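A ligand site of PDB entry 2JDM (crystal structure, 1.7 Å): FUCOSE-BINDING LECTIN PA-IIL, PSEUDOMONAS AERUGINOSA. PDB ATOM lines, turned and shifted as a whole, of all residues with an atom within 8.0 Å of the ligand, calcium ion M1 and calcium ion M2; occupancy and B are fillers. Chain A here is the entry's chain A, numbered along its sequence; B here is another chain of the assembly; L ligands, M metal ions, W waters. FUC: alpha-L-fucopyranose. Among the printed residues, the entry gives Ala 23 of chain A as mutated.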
ATOM      1  N   ALA A  21     -23.755  11.456 -31.138  1.00  0.00           N
ATOM      2  CA  ALA A  21     -22.735  11.345 -30.091  1.00  0.00           C
ATOM      3  C   ALA A  21     -21.384  11.935 -30.501  1.00  0.00           C
ATOM      4  O   ALA A  21     -20.956  11.798 -31.653  1.00  0.00           O
ATOM      5  CB  ALA A  21     -22.549   9.886 -29.688  1.00  0.00           C
ATOM      6  N   ASN A  22     -20.718  12.566 -29.531  1.00  0.00           N
ATOM      7  CA  ASN A  22     -19.396  13.135 -29.718  1.00  0.00           C
ATOM      8  C   ASN A  22     -18.574  13.014 -28.413  1.00  0.00           C
ATOM      9  O   ASN A  22     -18.302  14.020 -27.758  1.00  0.00           O
ATOM     10  CB  ASN A  22     -19.498  14.609 -30.127  1.00  0.00           C
ATOM     11  CG  ASN A  22     -20.051  14.791 -31.529  1.00  0.00           C
ATOM     12  OD1 ASN A  22     -19.345  14.561 -32.508  1.00  0.00           O
ATOM     13  ND2 ASN A  22     -21.329  15.220 -31.629  1.00  0.00           N
ATOM     14  N   ALA A  23     -18.230  11.778 -28.056  1.00  0.00           N
ATOM     15  CA  ALA A  23     -17.585  11.509 -26.755  1.00  0.00           C
ATOM     16  C   ALA A  23     -16.954  10.129 -26.705  1.00  0.00           C
ATOM     17  O   ALA A  23     -17.355   9.232 -27.460  1.00  0.00           O
ATOM     18  CB  ALA A  23     -18.606  11.668 -25.608  1.00  0.00           C
ATOM     19  N   SER A  24     -15.999   9.934 -25.792  1.00  0.00           N
ATOM     20  CA  SER A  24     -15.388   8.624 -25.638  1.00  0.00           C
ATOM     21  C   SER A  24     -16.396   7.575 -25.111  1.00  0.00           C
ATOM     22  O   SER A  24     -16.314   6.386 -25.479  1.00  0.00           O
ATOM     23  CB  SER A  24     -14.189   8.722 -24.683  1.00  0.00           C
ATOM     24  OG  SER A  24     -14.634   9.062 -23.386  1.00  0.00           O
ATOM     25  N   GLY A  25     -17.302   8.003 -24.229  1.00  0.00           N
ATOM     26  CA  GLY A  25     -18.212   7.084 -23.524  1.00  0.00           C
ATOM     27  C   GLY A  25     -19.565   6.914 -24.196  1.00  0.00           C
ATOM     28  O   GLY A  25     -20.034   7.814 -24.915  1.00  0.00           O
ATOM     29  N   GLN A  27     -23.307   7.097 -24.809  1.00  0.00           N
ATOM     30  CA  GLN A  27     -24.372   7.994 -24.372  1.00  0.00           C
ATOM     31  C   GLN A  27     -25.671   7.224 -24.314  1.00  0.00           C
ATOM     32  O   GLN A  27     -25.993   6.474 -25.232  1.00  0.00           O
ATOM     33  CB  GLN A  27     -24.541   9.153 -25.359  1.00  0.00           C
ATOM     34  CG  GLN A  27     -23.225   9.820 -25.742  1.00  0.00           C
ATOM     35  CD  GLN A  27     -22.653  10.693 -24.642  1.00  0.00           C
ATOM     36  OE1 GLN A  27     -23.328  11.610 -24.160  1.00  0.00           O
ATOM     37  NE2 GLN A  27     -21.406  10.422 -24.240  1.00  0.00           N
ATOM     38  N   GLN A  44     -22.160   5.130 -29.171  1.00  0.00           N
ATOM     39  CA  GLN A  44     -20.862   5.754 -28.904  1.00  0.00           C
ATOM     40  C   GLN A  44     -20.213   6.194 -30.208  1.00  0.00           C
ATOM     41  O   GLN A  44     -20.114   5.386 -31.138  1.00  0.00           O
ATOM     42  CB  GLN A  44     -19.935   4.745 -28.190  1.00  0.00           C
ATOM     43  CG  GLN A  44     -18.587   5.332 -27.733  1.00  0.00           C
ATOM     44  CD  GLN A  44     -17.604   5.469 -28.861  1.00  0.00           C
ATOM     45  OE1 GLN A  44     -17.416   4.539 -29.648  1.00  0.00           O
ATOM     46  NE2 GLN A  44     -16.981   6.646 -28.962  1.00  0.00           N
ATOM     47  N   SER A  45     -19.785   7.451 -30.251  1.00  0.00           N
ATOM     48  CA  SER A  45     -19.128   8.018 -31.438  1.00  0.00           C
ATOM     49  C   SER A  45     -18.383   9.259 -31.004  1.00  0.00           C
ATOM     50  O   SER A  45     -18.843   9.973 -30.116  1.00  0.00           O
ATOM     51  CB  SER A  45     -20.157   8.412 -32.509  1.00  0.00           C
ATOM     52  OG  SER A  45     -19.491   8.843 -33.699  1.00  0.00           O
ATOM     53  N   THR A  46     -17.254   9.511 -31.657  1.00  0.00           N
ATOM     54  CA  THR A  46     -16.565  10.767 -31.536  1.00  0.00           C
ATOM     55  C   THR A  46     -16.625  11.486 -32.888  1.00  0.00           C
ATOM     56  O   THR A  46     -15.867  12.418 -33.125  1.00  0.00           O
ATOM     57  CB  THR A  46     -15.091  10.591 -31.084  1.00  0.00           C
ATOM     58  OG1 THR A  46     -14.465   9.591 -31.915  1.00  0.00           O
ATOM     59  CG2 THR A  46     -15.024  10.119 -29.639  1.00  0.00           C
ATOM     60  N   VAL A  70     -24.321   9.119 -18.918  1.00  0.00           N
ATOM     61  CA  VAL A  70     -23.073   8.542 -19.409  1.00  0.00           C
ATOM     62  C   VAL A  70     -22.282   8.020 -18.198  1.00  0.00           C
ATOM     63  O   VAL A  70     -22.129   8.744 -17.210  1.00  0.00           O
ATOM     64  CB  VAL A  70     -22.213   9.617 -20.146  1.00  0.00           C
ATOM     65  CG1 VAL A  70     -20.879   9.041 -20.656  1.00  0.00           C
ATOM     66  CG2 VAL A  70     -22.995  10.232 -21.295  1.00  0.00           C
ATOM     67  N   SER A  95     -25.293  18.362 -24.265  1.00  0.00           N
ATOM     68  CA  SER A  95     -25.014  17.754 -22.968  1.00  0.00           C
ATOM     69  C   SER A  95     -23.521  17.591 -22.696  1.00  0.00           C
ATOM     70  O   SER A  95     -22.720  17.396 -23.638  1.00  0.00           O
ATOM     71  CB  SER A  95     -25.771  16.417 -22.832  1.00  0.00           C
ATOM     72  OG  SER A  95     -25.304  15.447 -23.780  1.00  0.00           O
ATOM     73  N   GLU A  96     -23.160  17.676 -21.414  1.00  0.00           N
ATOM     74  CA  GLU A  96     -21.761  17.572 -20.988  1.00  0.00           C
ATOM     75  C   GLU A  96     -21.574  16.442 -19.985  1.00  0.00           C
ATOM     76  O   GLU A  96     -22.145  16.457 -18.899  1.00  0.00           O
ATOM     77  CB  GLU A  96     -21.244  18.909 -20.388  1.00  0.00           C
ATOM     78  CG  GLU A  96     -19.766  18.884 -19.984  1.00  0.00           C
ATOM     79  CD  GLU A  96     -18.823  18.369 -21.095  1.00  0.00           C
ATOM     80  OE1 GLU A  96     -18.891  18.884 -22.247  1.00  0.00           O
ATOM     81  OE2 GLU A  96     -18.014  17.450 -20.819  1.00  0.00           O
ATOM     82  N   ASP A  97     -20.724  15.482 -20.329  1.00  0.00           N
ATOM     83  CA  ASP A  97     -20.569  14.280 -19.521  1.00  0.00           C
ATOM     84  C   ASP A  97     -19.256  14.288 -18.727  1.00  0.00           C
ATOM     85  O   ASP A  97     -19.002  13.375 -17.913  1.00  0.00           O
ATOM     86  CB  ASP A  97     -20.677  13.019 -20.393  1.00  0.00           C
ATOM     87  CG  ASP A  97     -19.478  12.813 -21.329  1.00  0.00           C
ATOM     88  OD1 ASP A  97     -18.383  13.358 -21.080  1.00  0.00           O
ATOM     89  OD2 ASP A  97     -19.631  12.067 -22.321  1.00  0.00           O
ATOM     90  N   GLY A  98     -18.454  15.326 -18.961  1.00  0.00           N
ATOM     91  CA  GLY A  98     -17.096  15.403 -18.464  1.00  0.00           C
ATOM     92  C   GLY A  98     -16.684  16.795 -18.040  1.00  0.00           C
ATOM     93  O   GLY A  98     -17.419  17.506 -17.348  1.00  0.00           O
ATOM     94  N   THR A  99     -15.488  17.163 -18.468  1.00  0.00           N
ATOM     95  CA  THR A  99     -14.808  18.318 -17.884  1.00  0.00           C
ATOM     96  C   THR A  99     -14.535  19.440 -18.890  1.00  0.00           C
ATOM     97  O   THR A  99     -14.321  20.569 -18.473  1.00  0.00           O
ATOM     98  CB  THR A  99     -13.485  17.908 -17.186  1.00  0.00           C
ATOM     99  OG1 THR A  99     -12.598  17.316 -18.138  1.00  0.00           O
ATOM    100  CG2 THR A  99     -13.754  16.888 -16.047  1.00  0.00           C
ATOM    101  N   ASP A 100     -14.540  19.136 -20.185  1.00  0.00           N
ATOM    102  CA  ASP A 100     -14.118  20.081 -21.231  1.00  0.00           C
ATOM    103  C   ASP A 100     -15.177  21.123 -21.663  1.00  0.00           C
ATOM    104  O   ASP A 100     -14.894  22.104 -22.349  1.00  0.00           O
ATOM    105  CB  ASP A 100     -13.563  19.343 -22.467  1.00  0.00           C
ATOM    106  CG  ASP A 100     -14.625  18.608 -23.274  1.00  0.00           C
ATOM    107  OD1 ASP A 100     -15.767  18.394 -22.789  1.00  0.00           O
ATOM    108  OD2 ASP A 100     -14.295  18.212 -24.421  1.00  0.00           O
ATOM    109  N   ASN A 101     -16.410  20.892 -21.239  1.00  0.00           N
ATOM    110  CA  ASN A 101     -17.514  21.812 -21.519  1.00  0.00           C
ATOM    111  C   ASN A 101     -17.750  22.117 -23.007  1.00  0.00           C
ATOM    112  O   ASN A 101     -18.127  23.234 -23.364  1.00  0.00           O
ATOM    113  CB  ASN A 101     -17.394  23.101 -20.699  1.00  0.00           C
ATOM    114  CG  ASN A 101     -17.396  22.817 -19.198  1.00  0.00           C
ATOM    115  OD1 ASN A 101     -18.094  21.932 -18.714  1.00  0.00           O
ATOM    116  ND2 ASN A 101     -16.585  23.571 -18.461  1.00  0.00           N
ATOM    117  N   ASP A 102     -17.526  21.125 -23.873  1.00  0.00           N
ATOM    118  CA  ASP A 102     -17.945  21.292 -25.281  1.00  0.00           C
ATOM    119  C   ASP A 102     -19.457  21.098 -25.503  1.00  0.00           C
ATOM    120  O   ASP A 102     -20.007  21.561 -26.511  1.00  0.00           O
ATOM    121  CB  ASP A 102     -17.079  20.455 -26.264  1.00  0.00           C
ATOM    122  CG  ASP A 102     -17.172  18.945 -26.044  1.00  0.00           C
ATOM    123  OD1 ASP A 102     -17.864  18.448 -25.120  1.00  0.00           O
ATOM    124  OD2 ASP A 102     -16.542  18.231 -26.867  1.00  0.00           O
ATOM    125  N   TYR A 103     -20.121  20.420 -24.587  1.00  0.00           N
ATOM    126  CA  TYR A 103     -21.583  20.282 -24.558  1.00  0.00           C
ATOM    127  C   TYR A 103     -22.178  19.568 -25.772  1.00  0.00           C
ATOM    128  O   TYR A 103     -23.353  19.737 -26.094  1.00  0.00           O
ATOM    129  CB  TYR A 103     -22.318  21.612 -24.231  1.00  0.00           C
ATOM    130  CG  TYR A 103     -22.366  21.827 -22.746  1.00  0.00           C
ATOM    131  CD1 TYR A 103     -23.440  21.387 -21.984  1.00  0.00           C
ATOM    132  CD2 TYR A 103     -21.285  22.415 -22.091  1.00  0.00           C
ATOM    133  CE1 TYR A 103     -23.457  21.559 -20.604  1.00  0.00           C
ATOM    134  CE2 TYR A 103     -21.288  22.578 -20.728  1.00  0.00           C
ATOM    135  CZ  TYR A 103     -22.358  22.163 -19.983  1.00  0.00           C
ATOM    136  OH  TYR A 103     -22.330  22.309 -18.626  1.00  0.00           O
ATOM    137  N   ASN A 104     -21.353  18.744 -26.416  1.00  0.00           N
ATOM    138  CA  ASN A 104     -21.744  18.101 -27.668  1.00  0.00           C
ATOM    139  C   ASN A 104     -21.745  16.603 -27.496  1.00  0.00           C
ATOM    140  O   ASN A 104     -21.923  15.862 -28.465  1.00  0.00           O
ATOM    141  CB  ASN A 104     -20.791  18.516 -28.817  1.00  0.00           C
ATOM    142  CG  ASN A 104     -19.450  17.822 -28.756  1.00  0.00           C
ATOM    143  OD1 ASN A 104     -19.151  17.073 -27.802  1.00  0.00           O
ATOM    144  ND2 ASN A 104     -18.624  18.038 -29.768  1.00  0.00           N
ATOM    145  N   ASP A 105     -21.553  16.150 -26.253  1.00  0.00           N
ATOM    146  CA  ASP A 105     -21.292  14.719 -26.005  1.00  0.00           C
ATOM    147  C   ASP A 105     -22.453  13.853 -26.459  1.00  0.00           C
ATOM    148  O   ASP A 105     -22.256  12.809 -27.061  1.00  0.00           O
ATOM    149  CB  ASP A 105     -20.915  14.460 -24.551  1.00  0.00           C
ATOM    150  CG  ASP A 105     -19.686  15.240 -24.136  1.00  0.00           C
ATOM    151  OD1 ASP A 105     -18.764  15.372 -24.985  1.00  0.00           O
ATOM    152  OD2 ASP A 105     -19.641  15.751 -23.005  1.00  0.00           O
ATOM    153  N   ALA A 106     -23.659  14.308 -26.132  1.00  0.00           N
ATOM    154  CA  ALA A 106     -24.848  13.855 -26.836  1.00  0.00           C
ATOM    155  C   ALA A 106     -25.597  15.124 -27.210  1.00  0.00           C
ATOM    156  O   ALA A 106     -25.839  15.992 -26.368  1.00  0.00           O
ATOM    157  CB  ALA A 106     -25.684  12.970 -25.995  1.00  0.00           C
ATOM    158  N   VAL A 107     -25.932  15.222 -28.496  1.00  0.00           N
ATOM    159  CA  VAL A 107     -26.642  16.366 -29.064  1.00  0.00           C
ATOM    160  C   VAL A 107     -28.000  15.823 -29.515  1.00  0.00           C
ATOM    161  O   VAL A 107     -28.031  14.809 -30.199  1.00  0.00           O
ATOM    162  CB  VAL A 107     -25.913  16.961 -30.291  1.00  0.00           C
ATOM    163  CG1 VAL A 107     -26.743  18.083 -30.970  1.00  0.00           C
ATOM    164  CG2 VAL A 107     -24.552  17.525 -29.901  1.00  0.00           C
ATOM    165  N   PRO B 113     -19.040  22.360 -32.442  1.00  0.00           N
ATOM    166  CA  PRO B 113     -17.999  21.447 -32.912  1.00  0.00           C
ATOM    167  C   PRO B 113     -18.344  19.981 -32.613  1.00  0.00           C
ATOM    168  O   PRO B 113     -19.313  19.680 -31.897  1.00  0.00           O
ATOM    169  CB  PRO B 113     -16.781  21.875 -32.104  1.00  0.00           C
ATOM    170  CG  PRO B 113     -17.376  22.323 -30.810  1.00  0.00           C
ATOM    171  CD  PRO B 113     -18.680  22.967 -31.148  1.00  0.00           C
ATOM    172  N   LEU B 114     -17.521  19.098 -33.161  1.00  0.00           N
ATOM    173  CA  LEU B 114     -17.660  17.669 -33.006  1.00  0.00           C
ATOM    174  C   LEU B 114     -16.529  17.139 -32.136  1.00  0.00           C
ATOM    175  O   LEU B 114     -15.666  17.906 -31.688  1.00  0.00           O
ATOM    176  CB  LEU B 114     -17.617  16.976 -34.378  1.00  0.00           C
ATOM    177  CG  LEU B 114     -18.555  17.468 -35.479  1.00  0.00           C
ATOM    178  CD1 LEU B 114     -18.374  16.602 -36.749  1.00  0.00           C
ATOM    179  CD2 LEU B 114     -20.002  17.514 -34.976  1.00  0.00           C
ATOM    180  N   GLY B 115     -16.547  15.840 -31.913  1.00  0.00           N
ATOM    181  CA  GLY B 115     -15.461  15.160 -31.187  1.00  0.00           C
ATOM    182  C   GLY B 115     -15.609  15.197 -29.685  1.00  0.00           C
ATOM    183  O   GLY B 115     -16.399  15.953 -29.113  1.00  0.00           O
ATOM    184  OXT GLY B 115     -14.885  14.445 -28.997  1.00  0.00           O
HETATM  185  C1  FUC L   1     -15.248  12.864 -23.390  1.00  0.00           C
HETATM  186  C2  FUC L   1     -15.995  14.166 -23.724  1.00  0.00           C
HETATM  187  C3  FUC L   1     -15.104  15.130 -24.477  1.00  0.00           C
HETATM  188  C4  FUC L   1     -14.554  14.454 -25.730  1.00  0.00           C
HETATM  189  C5  FUC L   1     -13.831  13.140 -25.333  1.00  0.00           C
HETATM  190  C6  FUC L   1     -13.351  12.371 -26.560  1.00  0.00           C
HETATM  191  O1  FUC L   1     -14.252  13.129 -22.426  1.00  0.00           O
HETATM  192  O2  FUC L   1     -16.511  14.841 -22.581  1.00  0.00           O
HETATM  193  O3  FUC L   1     -15.842  16.282 -24.863  1.00  0.00           O
HETATM  194  O4  FUC L   1     -15.611  14.219 -26.645  1.00  0.00           O
HETATM  195  O5  FUC L   1     -14.718  12.295 -24.588  1.00  0.00           O
HETATM  196 CA    CA M   1     -17.603  17.061 -23.253  1.00  0.00          CA
HETATM  197 CA    CA M   2     -17.356  15.934 -26.858  1.00  0.00          CA
HETATM  198  O   HOH W   1     -13.483  10.554 -21.580  1.00  0.00           O
HETATM  199  O   HOH W   2     -14.376  15.784 -20.604  1.00  0.00           O
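An oxygen (O5) of the ligand sits at hydrogen-bond distance from the backbone NH of Ser 24, 2.9 Å away.
OD1 of Asp 97 sits close to O2 of the ligand, at 2.8 Å.
The side-chain hydroxyl of Ser 24 sits at hydrogen-bond distance from an oxygen (O5) of the ligand.
The side-chain carboxylate (OE2) of Glu 96 lies close to the backbone NH (N) of Gly 98 (2.9 Å).
The side-chain amide nitrogen of Gln 44 sits at hydrogen-bond distance from the backbone carbonyl oxygen of Ala 23 (3.0 Å).
O of Ser 45 is in hydrogen-bond range of N of Ala 23, 2.8 Å away.
The backbone NH (N) of Asn 101 lies close to the side-chain carboxylate (OE1) of Glu 96.
N of Asn 22 lies close to O of Ser 45, at 3.3 Å.
OD2 of Asp 105 lies close to N of Asp 97 (2.9 Å).
N of Asn 104 lies within hydrogen-bond range of O of Ser 95 (3.4 Å).
The side-chain carboxylate (OE2) of Glu 96 sits close to the backbone NH (N) of Thr 99, at 3.5 Å.
Residues that only touch the ligand: Ala 23 (3.4 Å).
Of the 26 residues printed, 9 come within 4 Å of the ligand.
Within 4 Å of calcium ion M1: Glu 96, Asp 100, Asp 102 and Asp 105.
Along chain A the residues within 4 Å of calcium ion M1 span positions 96 to 105.
The nearest printed residue that does not touch calcium ion M1 is Asp 97 (4.4 Å).
Five residues have an atom within 4 Å of calcium ion M2: Asn 22, Asp 102, Asn 104, Asp 105 and Gly 115 of chain B.
Calcium ion M1 is bound by OD1 of Asp 100 (2.3 Å), OD1 of Asp 102 (2.3 Å), OD2 of Asp 105 (2.4 Å), OE1 of Glu 96 (2.4 Å), OE2 of Glu 96 (2.5 Å), O3 of the ligand (2.5 Å), O2 of the ligand (2.6 Å) and OD1 of Asp 105 (2.7 Å).
Calcium ion M2 is bound by O of Asn 22 (2.3 Å).
The side-chain amide oxygen (OD1) of Asn 104 binds calcium ion M2, 2.3 Å away.
The side-chain carboxylate (OD1) of Asp 105 binds calcium ion M2, at 2.4 Å.
The side-chain carboxylate (OD2) of Asp 102 is bound to calcium ion M2, 2.4 Å away.
O of Gly 115 of chain B is bound to calcium ion M2, 2.4 Å away.
Calcium ion M2 is bound by O4 of the ligand, at 2.5 Å.
O3 of the ligand is bound to calcium ion M2.
Calcium ion M2 has seven donor atoms within binding distance.
Slightly farther from calcium ion M2 lies the side-chain carboxylate (OD1) of Asp 102 (3.1 Å).
Water W1 lies within hydrogen-bond range of the side-chain hydroxyl of Ser 24 and an oxygen (O1) of the ligand.
Water W2 lies within hydrogen-bond range of the backbone NH (N) of Thr 99, an oxygen (O1) of the ligand and the backbone NH (N) of Asp 100.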
